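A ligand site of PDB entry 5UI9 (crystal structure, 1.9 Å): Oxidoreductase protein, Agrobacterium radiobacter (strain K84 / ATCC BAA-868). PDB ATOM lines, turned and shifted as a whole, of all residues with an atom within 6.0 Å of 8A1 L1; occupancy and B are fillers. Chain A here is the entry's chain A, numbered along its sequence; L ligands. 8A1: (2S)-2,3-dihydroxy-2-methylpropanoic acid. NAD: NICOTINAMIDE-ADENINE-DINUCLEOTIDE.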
ATOM      1  N   PHE A  16      18.400  -1.567 -16.415  1.00  0.00           N
ATOM      2  CA  PHE A  16      18.045  -2.430 -15.296  1.00  0.00           C
ATOM      3  C   PHE A  16      19.108  -3.460 -14.931  1.00  0.00           C
ATOM      4  O   PHE A  16      19.180  -3.872 -13.769  1.00  0.00           O
ATOM      5  CB  PHE A  16      16.697  -3.118 -15.520  1.00  0.00           C
ATOM      6  CG  PHE A  16      16.086  -3.626 -14.244  1.00  0.00           C
ATOM      7  CD1 PHE A  16      15.551  -2.735 -13.313  1.00  0.00           C
ATOM      8  CD2 PHE A  16      16.091  -4.979 -13.943  1.00  0.00           C
ATOM      9  CE1 PHE A  16      14.998  -3.188 -12.132  1.00  0.00           C
ATOM     10  CE2 PHE A  16      15.542  -5.442 -12.748  1.00  0.00           C
ATOM     11  CZ  PHE A  16      14.988  -4.551 -11.855  1.00  0.00           C
ATOM     12  N   LYS A  98      11.384 -10.131 -18.016  1.00  0.00           N
ATOM     13  CA  LYS A  98      10.066  -9.821 -18.553  1.00  0.00           C
ATOM     14  C   LYS A  98      10.195  -8.642 -19.530  1.00  0.00           C
ATOM     15  O   LYS A  98      11.212  -7.954 -19.504  1.00  0.00           O
ATOM     16  CB  LYS A  98       9.009  -9.526 -17.462  1.00  0.00           C
ATOM     17  CG  LYS A  98       9.390  -8.650 -16.270  1.00  0.00           C
ATOM     18  CD  LYS A  98       9.748  -7.196 -16.595  1.00  0.00           C
ATOM     19  CE  LYS A  98       8.583  -6.420 -17.179  1.00  0.00           C
ATOM     20  NZ  LYS A  98       8.852  -4.950 -17.198  1.00  0.00           N
ATOM     21  N   ASN A 126      10.055 -10.304 -10.676  1.00  0.00           N
ATOM     22  CA  ASN A 126      10.524 -10.007  -9.312  1.00  0.00           C
ATOM     23  C   ASN A 126       9.504  -9.340  -8.371  1.00  0.00           C
ATOM     24  O   ASN A 126       9.777  -9.215  -7.178  1.00  0.00           O
ATOM     25  CB  ASN A 126      11.883  -9.246  -9.323  1.00  0.00           C
ATOM     26  CG  ASN A 126      11.845  -7.920 -10.075  1.00  0.00           C
ATOM     27  OD1 ASN A 126      10.832  -7.241 -10.142  1.00  0.00           O
ATOM     28  ND2 ASN A 126      12.997  -7.530 -10.638  1.00  0.00           N
ATOM     29  N   PHE A 127       8.335  -8.960  -8.889  1.00  0.00           N
ATOM     30  CA  PHE A 127       7.328  -8.256  -8.057  1.00  0.00           C
ATOM     31  C   PHE A 127       6.777  -9.136  -6.950  1.00  0.00           C
ATOM     32  O   PHE A 127       6.697  -8.698  -5.810  1.00  0.00           O
ATOM     33  CB  PHE A 127       6.208  -7.664  -8.913  1.00  0.00           C
ATOM     34  CG  PHE A 127       6.463  -6.245  -9.347  1.00  0.00           C
ATOM     35  CD1 PHE A 127       7.628  -5.918 -10.015  1.00  0.00           C
ATOM     36  CD2 PHE A 127       5.529  -5.245  -9.098  1.00  0.00           C
ATOM     37  CE1 PHE A 127       7.873  -4.605 -10.412  1.00  0.00           C
ATOM     38  CE2 PHE A 127       5.756  -3.933  -9.497  1.00  0.00           C
ATOM     39  CZ  PHE A 127       6.925  -3.615 -10.151  1.00  0.00           C
ATOM     40  N   PHE A 155      -1.743  -0.705  -9.015  1.00  0.00           N
ATOM     41  CA  PHE A 155      -0.485   0.011  -9.194  1.00  0.00           C
ATOM     42  C   PHE A 155      -0.837   1.249  -9.994  1.00  0.00           C
ATOM     43  O   PHE A 155      -0.989   1.176 -11.231  1.00  0.00           O
ATOM     44  CB  PHE A 155       0.526  -0.875  -9.930  1.00  0.00           C
ATOM     45  CG  PHE A 155       1.920  -0.284 -10.040  1.00  0.00           C
ATOM     46  CD1 PHE A 155       2.220   0.697 -10.989  1.00  0.00           C
ATOM     47  CD2 PHE A 155       2.962  -0.759  -9.246  1.00  0.00           C
ATOM     48  CE1 PHE A 155       3.492   1.225 -11.099  1.00  0.00           C
ATOM     49  CE2 PHE A 155       4.245  -0.247  -9.357  1.00  0.00           C
ATOM     50  CZ  PHE A 155       4.502   0.752 -10.288  1.00  0.00           C
ATOM     51  N   VAL A 161       8.813   6.860 -15.510  1.00  0.00           N
ATOM     52  CA  VAL A 161       9.544   5.645 -15.957  1.00  0.00           C
ATOM     53  C   VAL A 161      10.211   5.814 -17.311  1.00  0.00           C
ATOM     54  O   VAL A 161      11.110   5.049 -17.647  1.00  0.00           O
ATOM     55  CB  VAL A 161       8.637   4.386 -16.087  1.00  0.00           C
ATOM     56  CG1 VAL A 161       8.372   3.755 -14.746  1.00  0.00           C
ATOM     57  CG2 VAL A 161       7.337   4.676 -16.860  1.00  0.00           C
ATOM     58  N   GLN A 165      13.762   4.399 -19.089  1.00  0.00           N
ATOM     59  CA  GLN A 165      13.305   3.378 -20.041  1.00  0.00           C
ATOM     60  C   GLN A 165      12.524   4.034 -21.199  1.00  0.00           C
ATOM     61  O   GLN A 165      11.323   3.830 -21.325  1.00  0.00           O
ATOM     62  CB  GLN A 165      12.437   2.340 -19.297  1.00  0.00           C
ATOM     63  CG  GLN A 165      13.199   1.562 -18.226  1.00  0.00           C
ATOM     64  CD  GLN A 165      12.309   0.823 -17.245  1.00  0.00           C
ATOM     65  OE1 GLN A 165      12.281   1.149 -16.054  1.00  0.00           O
ATOM     66  NE2 GLN A 165      11.569  -0.188 -17.737  1.00  0.00           N
ATOM     67  N   TYR A 167      12.105   3.585 -24.442  1.00  0.00           N
ATOM     68  CA  TYR A 167      11.319   2.659 -25.274  1.00  0.00           C
ATOM     69  C   TYR A 167       9.843   2.483 -24.865  1.00  0.00           C
ATOM     70  O   TYR A 167       8.987   2.219 -25.714  1.00  0.00           O
ATOM     71  CB  TYR A 167      11.999   1.266 -25.359  1.00  0.00           C
ATOM     72  CG  TYR A 167      12.253   0.612 -24.022  1.00  0.00           C
ATOM     73  CD1 TYR A 167      11.272  -0.161 -23.393  1.00  0.00           C
ATOM     74  CD2 TYR A 167      13.482   0.752 -23.370  1.00  0.00           C
ATOM     75  CE1 TYR A 167      11.497  -0.760 -22.161  1.00  0.00           C
ATOM     76  CE2 TYR A 167      13.719   0.161 -22.135  1.00  0.00           C
ATOM     77  CZ  TYR A 167      12.725  -0.596 -21.542  1.00  0.00           C
ATOM     78  OH  TYR A 167      12.970  -1.156 -20.325  1.00  0.00           O
ATOM     79  N   LEU A 168       9.552   2.645 -23.572  1.00  0.00           N
ATOM     80  CA  LEU A 168       8.185   2.569 -23.046  1.00  0.00           C
ATOM     81  C   LEU A 168       7.224   3.590 -23.679  1.00  0.00           C
ATOM     82  O   LEU A 168       6.026   3.327 -23.782  1.00  0.00           O
ATOM     83  CB  LEU A 168       8.184   2.725 -21.518  1.00  0.00           C
ATOM     84  CG  LEU A 168       8.877   1.632 -20.696  1.00  0.00           C
ATOM     85  CD1 LEU A 168       8.830   1.951 -19.207  1.00  0.00           C
ATOM     86  CD2 LEU A 168       8.291   0.248 -20.979  1.00  0.00           C
ATOM     87  N   PHE A 174       2.010  -0.735 -24.160  1.00  0.00           N
ATOM     88  CA  PHE A 174       2.802  -0.191 -23.052  1.00  0.00           C
ATOM     89  C   PHE A 174       2.429  -0.887 -21.732  1.00  0.00           C
ATOM     90  O   PHE A 174       3.021  -1.920 -21.418  1.00  0.00           O
ATOM     91  CB  PHE A 174       2.719   1.346 -23.000  1.00  0.00           C
ATOM     92  CG  PHE A 174       3.245   1.981 -21.722  1.00  0.00           C
ATOM     93  CD1 PHE A 174       4.367   1.480 -21.065  1.00  0.00           C
ATOM     94  CD2 PHE A 174       2.615   3.107 -21.201  1.00  0.00           C
ATOM     95  CE1 PHE A 174       4.831   2.072 -19.892  1.00  0.00           C
ATOM     96  CE2 PHE A 174       3.073   3.707 -20.028  1.00  0.00           C
ATOM     97  CZ  PHE A 174       4.183   3.184 -19.367  1.00  0.00           C
ATOM     98  N   ASP A 178       4.325  -4.026 -19.919  1.00  0.00           N
ATOM     99  CA  ASP A 178       5.443  -3.576 -19.104  1.00  0.00           C
ATOM    100  C   ASP A 178       5.224  -3.808 -17.608  1.00  0.00           C
ATOM    101  O   ASP A 178       6.131  -4.267 -16.901  1.00  0.00           O
ATOM    102  CB  ASP A 178       5.701  -2.085 -19.323  1.00  0.00           C
ATOM    103  CG  ASP A 178       6.771  -1.535 -18.396  1.00  0.00           C
ATOM    104  OD1 ASP A 178       7.872  -2.151 -18.333  1.00  0.00           O
ATOM    105  OD2 ASP A 178       6.522  -0.522 -17.710  1.00  0.00           O
ATOM    106  N   LEU A 179       4.039  -3.459 -17.129  1.00  0.00           N
ATOM    107  CA  LEU A 179       3.765  -3.336 -15.696  1.00  0.00           C
ATOM    108  C   LEU A 179       2.653  -4.261 -15.235  1.00  0.00           C
ATOM    109  O   LEU A 179       2.799  -4.949 -14.215  1.00  0.00           O
ATOM    110  CB  LEU A 179       3.475  -1.865 -15.382  1.00  0.00           C
ATOM    111  CG  LEU A 179       3.099  -1.423 -13.956  1.00  0.00           C
ATOM    112  CD1 LEU A 179       1.631  -1.665 -13.660  1.00  0.00           C
ATOM    113  CD2 LEU A 179       4.004  -2.049 -12.908  1.00  0.00           C
ATOM    114  N   HIS A 182       3.425  -7.710 -14.180  1.00  0.00           N
ATOM    115  CA  HIS A 182       3.741  -7.903 -12.772  1.00  0.00           C
ATOM    116  C   HIS A 182       2.484  -8.042 -11.916  1.00  0.00           C
ATOM    117  O   HIS A 182       2.391  -8.946 -11.085  1.00  0.00           O
ATOM    118  CB  HIS A 182       4.534  -6.722 -12.184  1.00  0.00           C
ATOM    119  CG  HIS A 182       5.884  -6.497 -12.797  1.00  0.00           C
ATOM    120  ND1 HIS A 182       6.878  -7.459 -12.777  1.00  0.00           N
ATOM    121  CD2 HIS A 182       6.413  -5.409 -13.384  1.00  0.00           C
ATOM    122  CE1 HIS A 182       7.957  -6.961 -13.352  1.00  0.00           C
ATOM    123  NE2 HIS A 182       7.706  -5.733 -13.740  1.00  0.00           N
ATOM    124  N   TYR A 232      -0.150   4.602 -15.336  1.00  0.00           N
ATOM    125  CA  TYR A 232       1.003   5.509 -15.270  1.00  0.00           C
ATOM    126  C   TYR A 232       0.597   6.981 -15.530  1.00  0.00           C
ATOM    127  O   TYR A 232       1.462   7.825 -15.822  1.00  0.00           O
ATOM    128  CB  TYR A 232       2.118   5.057 -16.220  1.00  0.00           C
ATOM    129  CG  TYR A 232       3.163   4.156 -15.564  1.00  0.00           C
ATOM    130  CD1 TYR A 232       3.890   4.605 -14.453  1.00  0.00           C
ATOM    131  CD2 TYR A 232       3.441   2.890 -16.065  1.00  0.00           C
ATOM    132  CE1 TYR A 232       4.856   3.797 -13.862  1.00  0.00           C
ATOM    133  CE2 TYR A 232       4.401   2.077 -15.468  1.00  0.00           C
ATOM    134  CZ  TYR A 232       5.100   2.543 -14.373  1.00  0.00           C
ATOM    135  OH  TYR A 232       6.055   1.752 -13.781  1.00  0.00           O
ATOM    136  N   PHE A 241       5.115   5.087  -6.387  1.00  0.00           N
ATOM    137  CA  PHE A 241       5.995   4.180  -7.135  1.00  0.00           C
ATOM    138  C   PHE A 241       7.071   3.579  -6.199  1.00  0.00           C
ATOM    139  O   PHE A 241       7.700   4.346  -5.468  1.00  0.00           O
ATOM    140  CB  PHE A 241       6.654   4.905  -8.317  1.00  0.00           C
ATOM    141  CG  PHE A 241       7.610   4.054  -9.120  1.00  0.00           C
ATOM    142  CD1 PHE A 241       8.956   3.964  -8.764  1.00  0.00           C
ATOM    143  CD2 PHE A 241       7.174   3.346 -10.237  1.00  0.00           C
ATOM    144  CE1 PHE A 241       9.845   3.174  -9.491  1.00  0.00           C
ATOM    145  CE2 PHE A 241       8.052   2.560 -10.972  1.00  0.00           C
ATOM    146  CZ  PHE A 241       9.391   2.477 -10.602  1.00  0.00           C
ATOM    147  N   TRP A 288      13.665   3.098  -6.151  1.00  0.00           N
ATOM    148  CA  TRP A 288      13.747   1.730  -6.715  1.00  0.00           C
ATOM    149  C   TRP A 288      14.031   0.624  -5.694  1.00  0.00           C
ATOM    150  O   TRP A 288      14.079  -0.564  -6.065  1.00  0.00           O
ATOM    151  CB  TRP A 288      14.810   1.685  -7.800  1.00  0.00           C
ATOM    152  CG  TRP A 288      14.442   2.452  -9.004  1.00  0.00           C
ATOM    153  CD1 TRP A 288      14.678   3.779  -9.228  1.00  0.00           C
ATOM    154  CD2 TRP A 288      13.760   1.962 -10.149  1.00  0.00           C
ATOM    155  NE1 TRP A 288      14.196   4.134 -10.468  1.00  0.00           N
ATOM    156  CE2 TRP A 288      13.624   3.036 -11.048  1.00  0.00           C
ATOM    157  CE3 TRP A 288      13.266   0.706 -10.514  1.00  0.00           C
ATOM    158  CZ2 TRP A 288      12.990   2.901 -12.293  1.00  0.00           C
ATOM    159  CZ3 TRP A 288      12.649   0.559 -11.752  1.00  0.00           C
ATOM    160  CH2 TRP A 288      12.515   1.659 -12.626  1.00  0.00           C
ATOM    161  N   ILE A 291      12.080  -2.799  -5.479  1.00  0.00           N
ATOM    162  CA  ILE A 291      12.377  -3.648  -6.643  1.00  0.00           C
ATOM    163  C   ILE A 291      13.786  -4.205  -6.529  1.00  0.00           C
ATOM    164  O   ILE A 291      14.027  -5.404  -6.777  1.00  0.00           O
ATOM    165  CB  ILE A 291      12.176  -2.870  -7.975  1.00  0.00           C
ATOM    166  CG1 ILE A 291      10.695  -2.534  -8.178  1.00  0.00           C
ATOM    167  CG2 ILE A 291      12.714  -3.668  -9.168  1.00  0.00           C
ATOM    168  CD1 ILE A 291      10.423  -1.613  -9.353  1.00  0.00           C
HETATM  169  OXT 8A1 L   1       9.701  -2.727 -12.898  1.00  0.00           O
HETATM  170  C   8A1 L   1       9.378  -2.788 -14.111  1.00  0.00           C
HETATM  171  O   8A1 L   1       9.299  -3.865 -14.736  1.00  0.00           O
HETATM  172  CA  8A1 L   1       9.030  -1.512 -14.843  1.00  0.00           C
HETATM  173  CB  8A1 L   1       7.513  -1.355 -14.754  1.00  0.00           C
HETATM  174  O1  8A1 L   1       7.088  -0.076 -15.244  1.00  0.00           O
HETATM  175  O2  8A1 L   1       9.447  -1.607 -16.213  1.00  0.00           O
HETATM  176  C3  8A1 L   1       9.771  -0.331 -14.212  1.00  0.00           C
HETATM  177  PA  NAD L   2      17.842  -1.138 -22.018  1.00  0.00           P
HETATM  178  O1A NAD L   2      17.525  -0.797 -23.460  1.00  0.00           O
HETATM  179  O2A NAD L   2      18.306  -0.062 -21.081  1.00  0.00           O
HETATM  180  O5B NAD L   2      18.936  -2.311 -22.008  1.00  0.00           O
HETATM  181  C5B NAD L   2      18.957  -3.359 -22.976  1.00  0.00           C
HETATM  182  C4B NAD L   2      20.419  -3.599 -23.330  1.00  0.00           C
HETATM  183  O4B NAD L   2      20.515  -4.820 -24.050  1.00  0.00           O
HETATM  184  C3B NAD L   2      21.007  -2.512 -24.211  1.00  0.00           C
HETATM  185  O3B NAD L   2      22.236  -2.052 -23.639  1.00  0.00           O
HETATM  186  C2B NAD L   2      21.200  -3.161 -25.566  1.00  0.00           C
HETATM  187  O2B NAD L   2      22.371  -2.670 -26.231  1.00  0.00           O
HETATM  188  C1B NAD L   2      21.321  -4.630 -25.213  1.00  0.00           C
HETATM  189  N9A NAD L   2      20.883  -5.624 -26.224  1.00  0.00           N
HETATM  190  C8A NAD L   2      19.711  -5.674 -26.874  1.00  0.00           C
HETATM  191  N7A NAD L   2      19.674  -6.767 -27.689  1.00  0.00           N
HETATM  192  C5A NAD L   2      20.821  -7.450 -27.528  1.00  0.00           C
HETATM  193  C6A NAD L   2      21.435  -8.685 -28.070  1.00  0.00           C
HETATM  194  N6A NAD L   2      20.805  -9.450 -28.973  1.00  0.00           N
HETATM  195  N1A NAD L   2      22.670  -9.028 -27.618  1.00  0.00           N
HETATM  196  C2A NAD L   2      23.347  -8.279 -26.711  1.00  0.00           C
HETATM  197  N3A NAD L   2      22.839  -7.153 -26.189  1.00  0.00           N
HETATM  198  C4A NAD L   2      21.617  -6.691 -26.548  1.00  0.00           C
HETATM  199  O3  NAD L   2      16.565  -1.889 -21.394  1.00  0.00           O
HETATM  200  PN  NAD L   2      16.233  -1.933 -19.821  1.00  0.00           P
HETATM  201  O1N NAD L   2      15.472  -0.689 -19.417  1.00  0.00           O
HETATM  202  O2N NAD L   2      17.470  -2.317 -19.058  1.00  0.00           O
HETATM  203  O5D NAD L   2      15.182  -3.137 -19.826  1.00  0.00           O
HETATM  204  C5D NAD L   2      15.594  -4.433 -20.235  1.00  0.00           C
HETATM  205  C4D NAD L   2      14.522  -5.426 -19.820  1.00  0.00           C
HETATM  206  O4D NAD L   2      14.384  -5.379 -18.399  1.00  0.00           O
HETATM  207  C3D NAD L   2      13.161  -5.084 -20.430  1.00  0.00           C
HETATM  208  O3D NAD L   2      12.575  -6.266 -20.993  1.00  0.00           O
HETATM  209  C2D NAD L   2      12.347  -4.556 -19.271  1.00  0.00           C
HETATM  210  O2D NAD L   2      10.970  -4.911 -19.341  1.00  0.00           O
HETATM  211  C1D NAD L   2      13.010  -5.211 -18.055  1.00  0.00           C
HETATM  212  N1N NAD L   2      12.874  -4.483 -16.777  1.00  0.00           N
HETATM  213  C2N NAD L   2      12.536  -5.211 -15.700  1.00  0.00           C
HETATM  214  C3N NAD L   2      12.385  -4.642 -14.447  1.00  0.00           C
HETATM  215  C7N NAD L   2      11.991  -5.534 -13.293  1.00  0.00           C
HETATM  216  O7N NAD L   2      12.409  -6.685 -13.271  1.00  0.00           O
HETATM  217  N7N NAD L   2      11.210  -5.064 -12.315  1.00  0.00           N
HETATM  218  C4N NAD L   2      12.599  -3.275 -14.305  1.00  0.00           C
HETATM  219  C5N NAD L   2      12.954  -2.522 -15.428  1.00  0.00           C
HETATM  220  C6N NAD L   2      13.103  -3.155 -16.666  1.00  0.00           C
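OXT of 8A1 L1 lies within hydrogen-bond range of N7N of NAD L2.
The side-chain hydroxyl of Tyr 167 lies within hydrogen-bond range of the side-chain amide nitrogen of Gln 165 (3.1 Å). The side-chain amino group (NZ) of Lys 98 lies within salt-bridge range of the side-chain carboxylate (OD1) of Asp 178, 3.2 Å away.
Residues that only touch 8A1 L1: Phe 127, Trp 288 and Ile 291. Hydrophobic or aromatic side chains that line 8A1 L1: Phe 127, His 182, Tyr 232, Trp 288 and Ile 291. Eight residues have an atom within 4 Å of 8A1 L1: Lys 98, Phe 127, Gln 165, Asp 178, His 182, Tyr 232, Trp 288 and Ile 291. The nearest printed residue that does not touch 8A1 L1 is Leu 179 (4.03 Å).
The side-chain amino group (NZ) of Lys 98 lies within salt-bridge range of an oxygen (O) of 8A1 L1 (2.7 Å). An oxygen (O) of 8A1 L1 is in hydrogen-bond range of a ring nitrogen (NE2) of His 182, at 2.6 Å. The side-chain hydroxyl of Tyr 232 is in hydrogen-bond range of an oxygen (O1) of 8A1 L1 (2.6 Å). NE2 of Gln 165 is in hydrogen-bond range of O2 of 8A1 L1. An oxygen (O1N) of NAD L2 sits at hydrogen-bond distance from the side-chain hydroxyl of Tyr 167 (2.7 Å). O of Lys 98 is in hydrogen-bond range of O3D of NAD L2 (2.6 Å). An oxygen (O7N) of NAD L2 is in hydrogen-bond range of the side-chain amide nitrogen (ND2) of Asn 126, 2.8 Å away. The backbone NH (N) of Phe 16 sits at hydrogen-bond distance from an oxygen (O2N) of NAD L2. O2D of NAD L2 is in hydrogen-bond range of NZ of Lys 98, at 3.0 Å. OD2 of Asp 178 is in hydrogen-bond range of O1 of 8A1 L1 (2.6 Å).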
